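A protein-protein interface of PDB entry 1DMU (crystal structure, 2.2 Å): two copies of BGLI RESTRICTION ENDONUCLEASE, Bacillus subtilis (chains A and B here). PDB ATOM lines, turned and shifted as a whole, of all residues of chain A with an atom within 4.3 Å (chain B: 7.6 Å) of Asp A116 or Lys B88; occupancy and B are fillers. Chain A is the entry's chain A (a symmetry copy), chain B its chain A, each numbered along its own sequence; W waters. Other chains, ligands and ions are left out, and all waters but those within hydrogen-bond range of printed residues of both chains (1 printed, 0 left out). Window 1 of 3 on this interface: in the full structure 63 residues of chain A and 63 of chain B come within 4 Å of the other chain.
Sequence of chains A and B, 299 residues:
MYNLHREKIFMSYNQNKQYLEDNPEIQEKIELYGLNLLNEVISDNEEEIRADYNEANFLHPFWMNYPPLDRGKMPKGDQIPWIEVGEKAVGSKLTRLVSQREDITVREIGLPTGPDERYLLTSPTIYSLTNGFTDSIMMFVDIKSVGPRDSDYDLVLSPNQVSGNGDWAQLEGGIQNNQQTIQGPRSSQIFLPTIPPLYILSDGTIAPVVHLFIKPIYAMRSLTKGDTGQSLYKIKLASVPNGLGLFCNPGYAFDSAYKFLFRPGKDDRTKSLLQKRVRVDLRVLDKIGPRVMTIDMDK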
ATOM      1  N   GLU A  87       1.531  -0.515 -12.963  1.00  0.00           N
ATOM      2  CA  GLU A  87       2.915  -0.200 -12.636  1.00  0.00           C
ATOM      3  C   GLU A  87       3.803  -0.137 -13.859  1.00  0.00           C
ATOM      4  O   GLU A  87       4.666   0.732 -13.974  1.00  0.00           O
ATOM      5  CB  GLU A  87       3.497  -1.240 -11.677  1.00  0.00           C
ATOM      6  CG  GLU A  87       2.990  -1.120 -10.268  1.00  0.00           C
ATOM      7  CD  GLU A  87       3.631  -2.122  -9.323  1.00  0.00           C
ATOM      8  OE1 GLU A  87       4.024  -3.214  -9.779  1.00  0.00           O
ATOM      9  OE2 GLU A  87       3.737  -1.821  -8.118  1.00  0.00           O
ATOM     10  N   GLU A 108      19.406   7.486 -12.683  1.00  0.00           N
ATOM     11  CA  GLU A 108      18.873   6.590 -11.654  1.00  0.00           C
ATOM     12  C   GLU A 108      19.813   6.493 -10.470  1.00  0.00           C
ATOM     13  O   GLU A 108      20.622   5.595 -10.394  1.00  0.00           O
ATOM     14  CB  GLU A 108      18.634   5.192 -12.231  1.00  0.00           C
ATOM     15  CG  GLU A 108      17.627   5.153 -13.392  1.00  0.00           C
ATOM     16  CD  GLU A 108      18.228   5.575 -14.739  1.00  0.00           C
ATOM     17  OE1 GLU A 108      17.485   5.533 -15.738  1.00  0.00           O
ATOM     18  OE2 GLU A 108      19.423   5.950 -14.804  1.00  0.00           O
ATOM     19  N   PRO A 115       9.769   5.072  -3.376  1.00  0.00           N
ATOM     20  CA  PRO A 115       8.648   4.771  -4.267  1.00  0.00           C
ATOM     21  C   PRO A 115       8.979   3.932  -5.518  1.00  0.00           C
ATOM     22  O   PRO A 115      10.138   3.626  -5.789  1.00  0.00           O
ATOM     23  CB  PRO A 115       8.121   6.155  -4.620  1.00  0.00           C
ATOM     24  CG  PRO A 115       9.344   7.006  -4.618  1.00  0.00           C
ATOM     25  CD  PRO A 115      10.179   6.485  -3.489  1.00  0.00           C
ATOM     26  N   ASP A 116       7.941   3.562  -6.262  1.00  0.00           N
ATOM     27  CA  ASP A 116       8.066   2.770  -7.482  1.00  0.00           C
ATOM     28  C   ASP A 116       9.140   3.300  -8.412  1.00  0.00           C
ATOM     29  O   ASP A 116      10.032   2.561  -8.819  1.00  0.00           O
ATOM     30  CB  ASP A 116       6.738   2.747  -8.249  1.00  0.00           C
ATOM     31  CG  ASP A 116       5.670   1.957  -7.545  1.00  0.00           C
ATOM     32  OD1 ASP A 116       6.020   1.130  -6.677  1.00  0.00           O
ATOM     33  OD2 ASP A 116       4.479   2.155  -7.858  1.00  0.00           O
ATOM     34  N   GLU A 117       9.049   4.581  -8.761  1.00  0.00           N
ATOM     35  CA  GLU A 117      10.020   5.197  -9.666  1.00  0.00           C
ATOM     36  C   GLU A 117      10.797   6.310  -8.971  1.00  0.00           C
ATOM     37  O   GLU A 117      10.221   7.125  -8.240  1.00  0.00           O
ATOM     38  CB  GLU A 117       9.301   5.758 -10.907  1.00  0.00           C
ATOM     39  CG  GLU A 117       8.419   4.726 -11.654  1.00  0.00           C
ATOM     40  CD  GLU A 117       9.232   3.623 -12.362  1.00  0.00           C
ATOM     41  OE1 GLU A 117      10.397   3.852 -12.752  1.00  0.00           O
ATOM     42  OE2 GLU A 117       8.703   2.513 -12.521  1.00  0.00           O
ATOM     43  N   ARG A 118      12.114   6.321  -9.169  1.00  0.00           N
ATOM     44  CA  ARG A 118      12.962   7.364  -8.600  1.00  0.00           C
ATOM     45  C   ARG A 118      14.102   7.706  -9.555  1.00  0.00           C
ATOM     46  O   ARG A 118      14.788   6.820 -10.073  1.00  0.00           O
ATOM     47  CB  ARG A 118      13.570   6.949  -7.260  1.00  0.00           C
ATOM     48  CG  ARG A 118      12.719   6.048  -6.439  1.00  0.00           C
ATOM     49  CD  ARG A 118      13.285   5.961  -5.060  1.00  0.00           C
ATOM     50  NE  ARG A 118      14.285   4.903  -4.925  1.00  0.00           N
ATOM     51  CZ  ARG A 118      14.011   3.625  -4.673  1.00  0.00           C
ATOM     52  NH1 ARG A 118      12.754   3.214  -4.535  1.00  0.00           N
ATOM     53  NH2 ARG A 118      15.004   2.761  -4.498  1.00  0.00           N
ATOM     54  N   VAL A 141       7.993   9.027  -7.807  1.00  0.00           N
ATOM     55  CA  VAL A 141       6.673   8.736  -8.365  1.00  0.00           C
ATOM     56  C   VAL A 141       6.202   7.349  -7.992  1.00  0.00           C
ATOM     57  O   VAL A 141       6.910   6.361  -8.158  1.00  0.00           O
ATOM     58  CB  VAL A 141       6.681   8.850  -9.938  1.00  0.00           C
ATOM     59  CG1 VAL A 141       5.259   9.011 -10.463  1.00  0.00           C
ATOM     60  CG2 VAL A 141       7.549  10.044 -10.385  1.00  0.00           C
ATOM     61  N   ASP A 142       4.994   7.269  -7.472  1.00  0.00           N
ATOM     62  CA  ASP A 142       4.466   5.968  -7.124  1.00  0.00           C
ATOM     63  C   ASP A 142       3.087   5.784  -7.770  1.00  0.00           C
ATOM     64  O   ASP A 142       2.262   6.692  -7.760  1.00  0.00           O
ATOM     65  CB  ASP A 142       4.417   5.813  -5.594  1.00  0.00           C
ATOM     66  CG  ASP A 142       4.451   4.364  -5.161  1.00  0.00           C
ATOM     67  OD1 ASP A 142       3.367   3.778  -5.040  1.00  0.00           O
ATOM     68  OD2 ASP A 142       5.551   3.807  -4.949  1.00  0.00           O
ATOM     69  N   ILE A 143       2.883   4.608  -8.356  1.00  0.00           N
ATOM     70  CA  ILE A 143       1.644   4.234  -9.027  1.00  0.00           C
ATOM     71  C   ILE A 143       0.693   3.568  -8.032  1.00  0.00           C
ATOM     72  O   ILE A 143       1.064   2.594  -7.369  1.00  0.00           O
ATOM     73  CB  ILE A 143       1.929   3.233 -10.169  1.00  0.00           C
ATOM     74  CG1 ILE A 143       2.641   3.947 -11.311  1.00  0.00           C
ATOM     75  CG2 ILE A 143       0.630   2.631 -10.683  1.00  0.00           C
ATOM     76  CD1 ILE A 143       1.700   4.776 -12.175  1.00  0.00           C
ATOM     77  N   ASP B  52      26.105   5.580 -10.178  1.00  0.00           N
ATOM     78  CA  ASP B  52      24.751   5.687  -9.623  1.00  0.00           C
ATOM     79  C   ASP B  52      24.471   4.576  -8.623  1.00  0.00           C
ATOM     80  O   ASP B  52      23.658   4.749  -7.716  1.00  0.00           O
ATOM     81  CB  ASP B  52      23.711   5.698 -10.740  1.00  0.00           C
ATOM     82  CG  ASP B  52      23.760   6.993 -11.525  1.00  0.00           C
ATOM     83  OD1 ASP B  52      24.473   7.894 -11.057  1.00  0.00           O
ATOM     84  OD2 ASP B  52      23.118   7.122 -12.589  1.00  0.00           O
ATOM     85  N   TYR B  53      25.150   3.446  -8.776  1.00  0.00           N
ATOM     86  CA  TYR B  53      24.975   2.346  -7.837  1.00  0.00           C
ATOM     87  C   TYR B  53      25.632   2.750  -6.501  1.00  0.00           C
ATOM     88  O   TYR B  53      24.965   2.910  -5.485  1.00  0.00           O
ATOM     89  CB  TYR B  53      25.632   1.064  -8.376  1.00  0.00           C
ATOM     90  CG  TYR B  53      25.364  -0.170  -7.526  1.00  0.00           C
ATOM     91  CD1 TYR B  53      24.327  -1.049  -7.848  1.00  0.00           C
ATOM     92  CD2 TYR B  53      26.147  -0.458  -6.401  1.00  0.00           C
ATOM     93  CE1 TYR B  53      24.073  -2.170  -7.081  1.00  0.00           C
ATOM     94  CE2 TYR B  53      25.901  -1.583  -5.623  1.00  0.00           C
ATOM     95  CZ  TYR B  53      24.857  -2.437  -5.970  1.00  0.00           C
ATOM     96  OH  TYR B  53      24.585  -3.557  -5.199  1.00  0.00           O
ATOM     97  N   TRP B  82      20.216  -4.443   0.448  1.00  0.00           N
ATOM     98  CA  TRP B  82      20.603  -3.723  -0.771  1.00  0.00           C
ATOM     99  C   TRP B  82      19.801  -3.998  -2.040  1.00  0.00           C
ATOM    100  O   TRP B  82      20.193  -3.574  -3.126  1.00  0.00           O
ATOM    101  CB  TRP B  82      22.091  -3.998  -1.033  1.00  0.00           C
ATOM    102  CG  TRP B  82      22.940  -2.782  -1.316  1.00  0.00           C
ATOM    103  CD1 TRP B  82      23.909  -2.680  -2.261  1.00  0.00           C
ATOM    104  CD2 TRP B  82      22.925  -1.517  -0.621  1.00  0.00           C
ATOM    105  NE1 TRP B  82      24.505  -1.445  -2.207  1.00  0.00           N
ATOM    106  CE2 TRP B  82      23.923  -0.709  -1.211  1.00  0.00           C
ATOM    107  CE3 TRP B  82      22.169  -0.992   0.444  1.00  0.00           C
ATOM    108  CZ2 TRP B  82      24.189   0.596  -0.779  1.00  0.00           C
ATOM    109  CZ3 TRP B  82      22.433   0.309   0.873  1.00  0.00           C
ATOM    110  CH2 TRP B  82      23.440   1.088   0.258  1.00  0.00           C
ATOM    111  N   ILE B  83      18.674  -4.686  -1.888  1.00  0.00           N
ATOM    112  CA  ILE B  83      17.791  -5.053  -2.988  1.00  0.00           C
ATOM    113  C   ILE B  83      17.440  -3.960  -4.003  1.00  0.00           C
ATOM    114  O   ILE B  83      17.605  -4.153  -5.204  1.00  0.00           O
ATOM    115  CB  ILE B  83      16.444  -5.625  -2.449  1.00  0.00           C
ATOM    116  CG1 ILE B  83      16.702  -6.706  -1.403  1.00  0.00           C
ATOM    117  CG2 ILE B  83      15.630  -6.269  -3.590  1.00  0.00           C
ATOM    118  CD1 ILE B  83      15.453  -7.024  -0.549  1.00  0.00           C
ATOM    119  N   GLU B  84      16.938  -2.827  -3.530  1.00  0.00           N
ATOM    120  CA  GLU B  84      16.513  -1.754  -4.423  1.00  0.00           C
ATOM    121  C   GLU B  84      17.625  -0.965  -5.101  1.00  0.00           C
ATOM    122  O   GLU B  84      17.400  -0.362  -6.154  1.00  0.00           O
ATOM    123  CB  GLU B  84      15.556  -0.799  -3.686  1.00  0.00           C
ATOM    124  CG  GLU B  84      14.422  -1.501  -2.918  1.00  0.00           C
ATOM    125  CD  GLU B  84      13.334  -0.539  -2.460  1.00  0.00           C
ATOM    126  OE1 GLU B  84      13.431   0.666  -2.781  1.00  0.00           O
ATOM    127  OE2 GLU B  84      12.380  -0.987  -1.784  1.00  0.00           O
ATOM    128  N   VAL B  85      18.818  -0.958  -4.521  1.00  0.00           N
ATOM    129  CA  VAL B  85      19.915  -0.231  -5.149  1.00  0.00           C
ATOM    130  C   VAL B  85      20.247  -0.878  -6.505  1.00  0.00           C
ATOM    131  O   VAL B  85      20.382  -0.178  -7.515  1.00  0.00           O
ATOM    132  CB  VAL B  85      21.153  -0.197  -4.241  1.00  0.00           C
ATOM    133  CG1 VAL B  85      22.248   0.653  -4.886  1.00  0.00           C
ATOM    134  CG2 VAL B  85      20.769   0.378  -2.880  1.00  0.00           C
ATOM    135  N   GLY B  86      20.352  -2.211  -6.518  1.00  0.00           N
ATOM    136  CA  GLY B  86      20.635  -2.934  -7.743  1.00  0.00           C
ATOM    137  C   GLY B  86      19.460  -2.893  -8.712  1.00  0.00           C
ATOM    138  O   GLY B  86      19.639  -2.856  -9.930  1.00  0.00           O
ATOM    139  N   GLU B  87      18.241  -2.870  -8.178  1.00  0.00           N
ATOM    140  CA  GLU B  87      17.052  -2.850  -9.018  1.00  0.00           C
ATOM    141  C   GLU B  87      16.935  -1.582  -9.834  1.00  0.00           C
ATOM    142  O   GLU B  87      16.559  -1.612 -11.004  1.00  0.00           O
ATOM    143  CB  GLU B  87      15.786  -2.990  -8.170  1.00  0.00           C
ATOM    144  CG  GLU B  87      15.559  -4.377  -7.639  1.00  0.00           C
ATOM    145  CD  GLU B  87      14.264  -4.503  -6.855  1.00  0.00           C
ATOM    146  OE1 GLU B  87      13.818  -3.502  -6.260  1.00  0.00           O
ATOM    147  OE2 GLU B  87      13.691  -5.610  -6.826  1.00  0.00           O
ATOM    148  N   LYS B  88      17.257  -0.459  -9.212  1.00  0.00           N
ATOM    149  CA  LYS B  88      17.132   0.821  -9.882  1.00  0.00           C
ATOM    150  C   LYS B  88      18.397   1.262 -10.612  1.00  0.00           C
ATOM    151  O   LYS B  88      18.365   1.518 -11.811  1.00  0.00           O
ATOM    152  CB  LYS B  88      16.691   1.891  -8.854  1.00  0.00           C
ATOM    153  CG  LYS B  88      15.240   1.719  -8.339  1.00  0.00           C
ATOM    154  CD  LYS B  88      14.255   2.140  -9.430  1.00  0.00           C
ATOM    155  CE  LYS B  88      12.829   1.650  -9.212  1.00  0.00           C
ATOM    156  NZ  LYS B  88      12.045   1.738 -10.519  1.00  0.00           N
ATOM    157  N   ALA B  89      19.509   1.331  -9.891  1.00  0.00           N
ATOM    158  CA  ALA B  89      20.766   1.774 -10.471  1.00  0.00           C
ATOM    159  C   ALA B  89      21.249   0.846 -11.579  1.00  0.00           C
ATOM    160  O   ALA B  89      21.985   1.269 -12.476  1.00  0.00           O
ATOM    161  CB  ALA B  89      21.818   1.910  -9.383  1.00  0.00           C
ATOM    162  N   VAL B  90      20.855  -0.422 -11.517  1.00  0.00           N
ATOM    163  CA  VAL B  90      21.260  -1.338 -12.561  1.00  0.00           C
ATOM    164  C   VAL B  90      20.085  -1.763 -13.433  1.00  0.00           C
ATOM    165  O   VAL B  90      20.074  -1.493 -14.634  1.00  0.00           O
ATOM    166  CB  VAL B  90      22.001  -2.595 -11.997  1.00  0.00           C
ATOM    167  CG1 VAL B  90      22.431  -3.519 -13.162  1.00  0.00           C
ATOM    168  CG2 VAL B  90      23.251  -2.151 -11.223  1.00  0.00           C
ATOM    169  N   GLY B  91      19.087  -2.395 -12.833  1.00  0.00           N
ATOM    170  CA  GLY B  91      17.939  -2.865 -13.597  1.00  0.00           C
ATOM    171  C   GLY B  91      17.150  -1.824 -14.375  1.00  0.00           C
ATOM    172  O   GLY B  91      16.951  -1.950 -15.590  1.00  0.00           O
ATOM    173  N   SER B  92      16.692  -0.783 -13.691  1.00  0.00           N
ATOM    174  CA  SER B  92      15.895   0.233 -14.367  1.00  0.00           C
ATOM    175  C   SER B  92      16.711   1.065 -15.335  1.00  0.00           C
ATOM    176  O   SER B  92      16.211   1.478 -16.376  1.00  0.00           O
ATOM    177  CB  SER B  92      15.224   1.148 -13.343  1.00  0.00           C
ATOM    178  OG  SER B  92      14.111   0.499 -12.772  1.00  0.00           O
ATOM    179  N   LYS B  93      17.963   1.316 -14.972  1.00  0.00           N
ATOM    180  CA  LYS B  93      18.843   2.106 -15.810  1.00  0.00           C
ATOM    181  C   LYS B  93      19.068   1.410 -17.154  1.00  0.00           C
ATOM    182  O   LYS B  93      19.074   2.055 -18.215  1.00  0.00           O
ATOM    183  CB  LYS B  93      20.180   2.325 -15.104  1.00  0.00           C
ATOM    184  CG  LYS B  93      21.152   3.168 -15.897  1.00  0.00           C
ATOM    185  CD  LYS B  93      22.468   3.291 -15.157  1.00  0.00           C
ATOM    186  CE  LYS B  93      22.352   4.193 -13.926  1.00  0.00           C
ATOM    187  NZ  LYS B  93      22.186   5.623 -14.296  1.00  0.00           N
ATOM    188  N   LEU B  94      19.240   0.090 -17.104  1.00  0.00           N
ATOM    189  CA  LEU B  94      19.464  -0.693 -18.310  1.00  0.00           C
ATOM    190  C   LEU B  94      18.257  -0.646 -19.244  1.00  0.00           C
ATOM    191  O   LEU B  94      18.399  -0.535 -20.465  1.00  0.00           O
ATOM    192  CB  LEU B  94      19.810  -2.140 -17.934  1.00  0.00           C
ATOM    193  CG  LEU B  94      21.253  -2.336 -17.421  1.00  0.00           C
ATOM    194  CD1 LEU B  94      21.641  -3.811 -17.483  1.00  0.00           C
ATOM    195  CD2 LEU B  94      22.233  -1.523 -18.269  1.00  0.00           C
ATOM    196  N   THR B  95      17.061  -0.713 -18.679  1.00  0.00           N
ATOM    197  CA  THR B  95      15.873  -0.661 -19.512  1.00  0.00           C
ATOM    198  C   THR B  95      15.876   0.642 -20.320  1.00  0.00           C
ATOM    199  O   THR B  95      15.597   0.627 -21.512  1.00  0.00           O
ATOM    200  CB  THR B  95      14.584  -0.783 -18.650  1.00  0.00           C
ATOM    201  OG1 THR B  95      14.516  -2.107 -18.094  1.00  0.00           O
ATOM    202  CG2 THR B  95      13.350  -0.534 -19.486  1.00  0.00           C
ATOM    203  N   GLU B 117      11.673  -6.327 -14.890  1.00  0.00           N
ATOM    204  CA  GLU B 117      11.510  -5.550 -16.119  1.00  0.00           C
ATOM    205  C   GLU B 117      10.889  -6.393 -17.229  1.00  0.00           C
ATOM    206  O   GLU B 117      11.265  -7.554 -17.428  1.00  0.00           O
ATOM    207  CB  GLU B 117      12.873  -5.001 -16.579  1.00  0.00           C
ATOM    208  CG  GLU B 117      13.629  -4.185 -15.500  1.00  0.00           C
ATOM    209  CD  GLU B 117      12.958  -2.836 -15.169  1.00  0.00           C
ATOM    210  OE1 GLU B 117      12.266  -2.250 -16.028  1.00  0.00           O
ATOM    211  OE2 GLU B 117      13.118  -2.364 -14.035  1.00  0.00           O
ATOM    212  N   ILE B 143      16.528  -8.618 -11.828  1.00  0.00           N
ATOM    213  CA  ILE B 143      17.747  -8.278 -11.104  1.00  0.00           C
ATOM    214  C   ILE B 143      17.835  -9.102  -9.817  1.00  0.00           C
ATOM    215  O   ILE B 143      16.905  -9.092  -9.004  1.00  0.00           O
ATOM    216  CB  ILE B 143      17.749  -6.782 -10.722  1.00  0.00           C
ATOM    217  CG1 ILE B 143      17.942  -5.934 -11.972  1.00  0.00           C
ATOM    218  CG2 ILE B 143      18.870  -6.488  -9.735  1.00  0.00           C
ATOM    219  CD1 ILE B 143      19.389  -5.889 -12.445  1.00  0.00           C
HETATM  220  O   HOH W   1       9.419  -0.271 -10.039  1.00  0.00           O
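3 positions are printed for both chains.
Among the printed residues, merely in contact across the chains: Glu A108 with Asp B52, Glu A108 with Lys B88, Glu A108 with Ala B89 and Arg A118 with Lys B88.
Asp A116 touches one residue of chain B.
Of the printed residues of chain A, Lys B88 touches Glu A108, Asp A116, Glu A117 and Arg A118.
Of the printed residues of chain A, Ala B89 touches Glu A108.
Printed residues of chain B within 4 Å of Glu A108: Asp B52 (3.1 Å), Lys B88 (3.7 Å), Ala B89 (3.8 Å) and Lys B93 (2.8 Å).
Of the printed residues of chain A, Glu B84 touches Arg A118 (3.1 Å).
Printed residues of chain A within 4 Å of Asp B52: Glu A108 (3.1 Å).
Ile A143 touches none of the printed residues of chain B.
The nearest residue of chain B that does not touch Asp A116 is Ser B92 (6.0 Å).
The nearest printed residue of chain A that does not touch Lys B88 is Pro A115 (4.8 Å).
The nearest printed residue of chain A that does not touch Glu B84 is Pro A115 (5.4 Å).
The side-chain carboxylate of Asp B52 lies within salt-bridge range of the side-chain amino group of Lys B93 (2.5 Å).
The side-chain amino group of Lys B88 is in hydrogen-bond range of the side-chain hydroxyl of Ser B92 (3.3 Å).
The backbone carbonyl oxygen of Lys B88 is in hydrogen-bond range of the backbone NH of Lys B93 (3.2 Å).
NH1 of Arg A118 is in hydrogen-bond range of O of Pro A115 (2.9 Å).
The backbone NH (N) of Glu A117 sits at hydrogen-bond distance from the backbone carbonyl oxygen (O) of Val A141.
Water W1 lies within hydrogen-bond range of O of Asp A116 (3.1 Å) and NZ of Lys B88 (3.3 Å).
Among the printed residues, 8 pairs touch across the chains.
OE1 of Glu B84 is in salt-bridge range of NH2 of Arg A118, 3.1 Å away.
NZ of Lys B88 is in hydrogen-bond range of O of Asp A116 (2.8 Å).
The side-chain carboxylate (OE1) of Glu A117 is in salt-bridge range of the side-chain amino group (NZ) of Lys B88.
The side-chain amino group (NZ) of Lys B93 is in salt-bridge range of the side-chain carboxylate (OE2) of Glu A108, 2.8 Å away.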
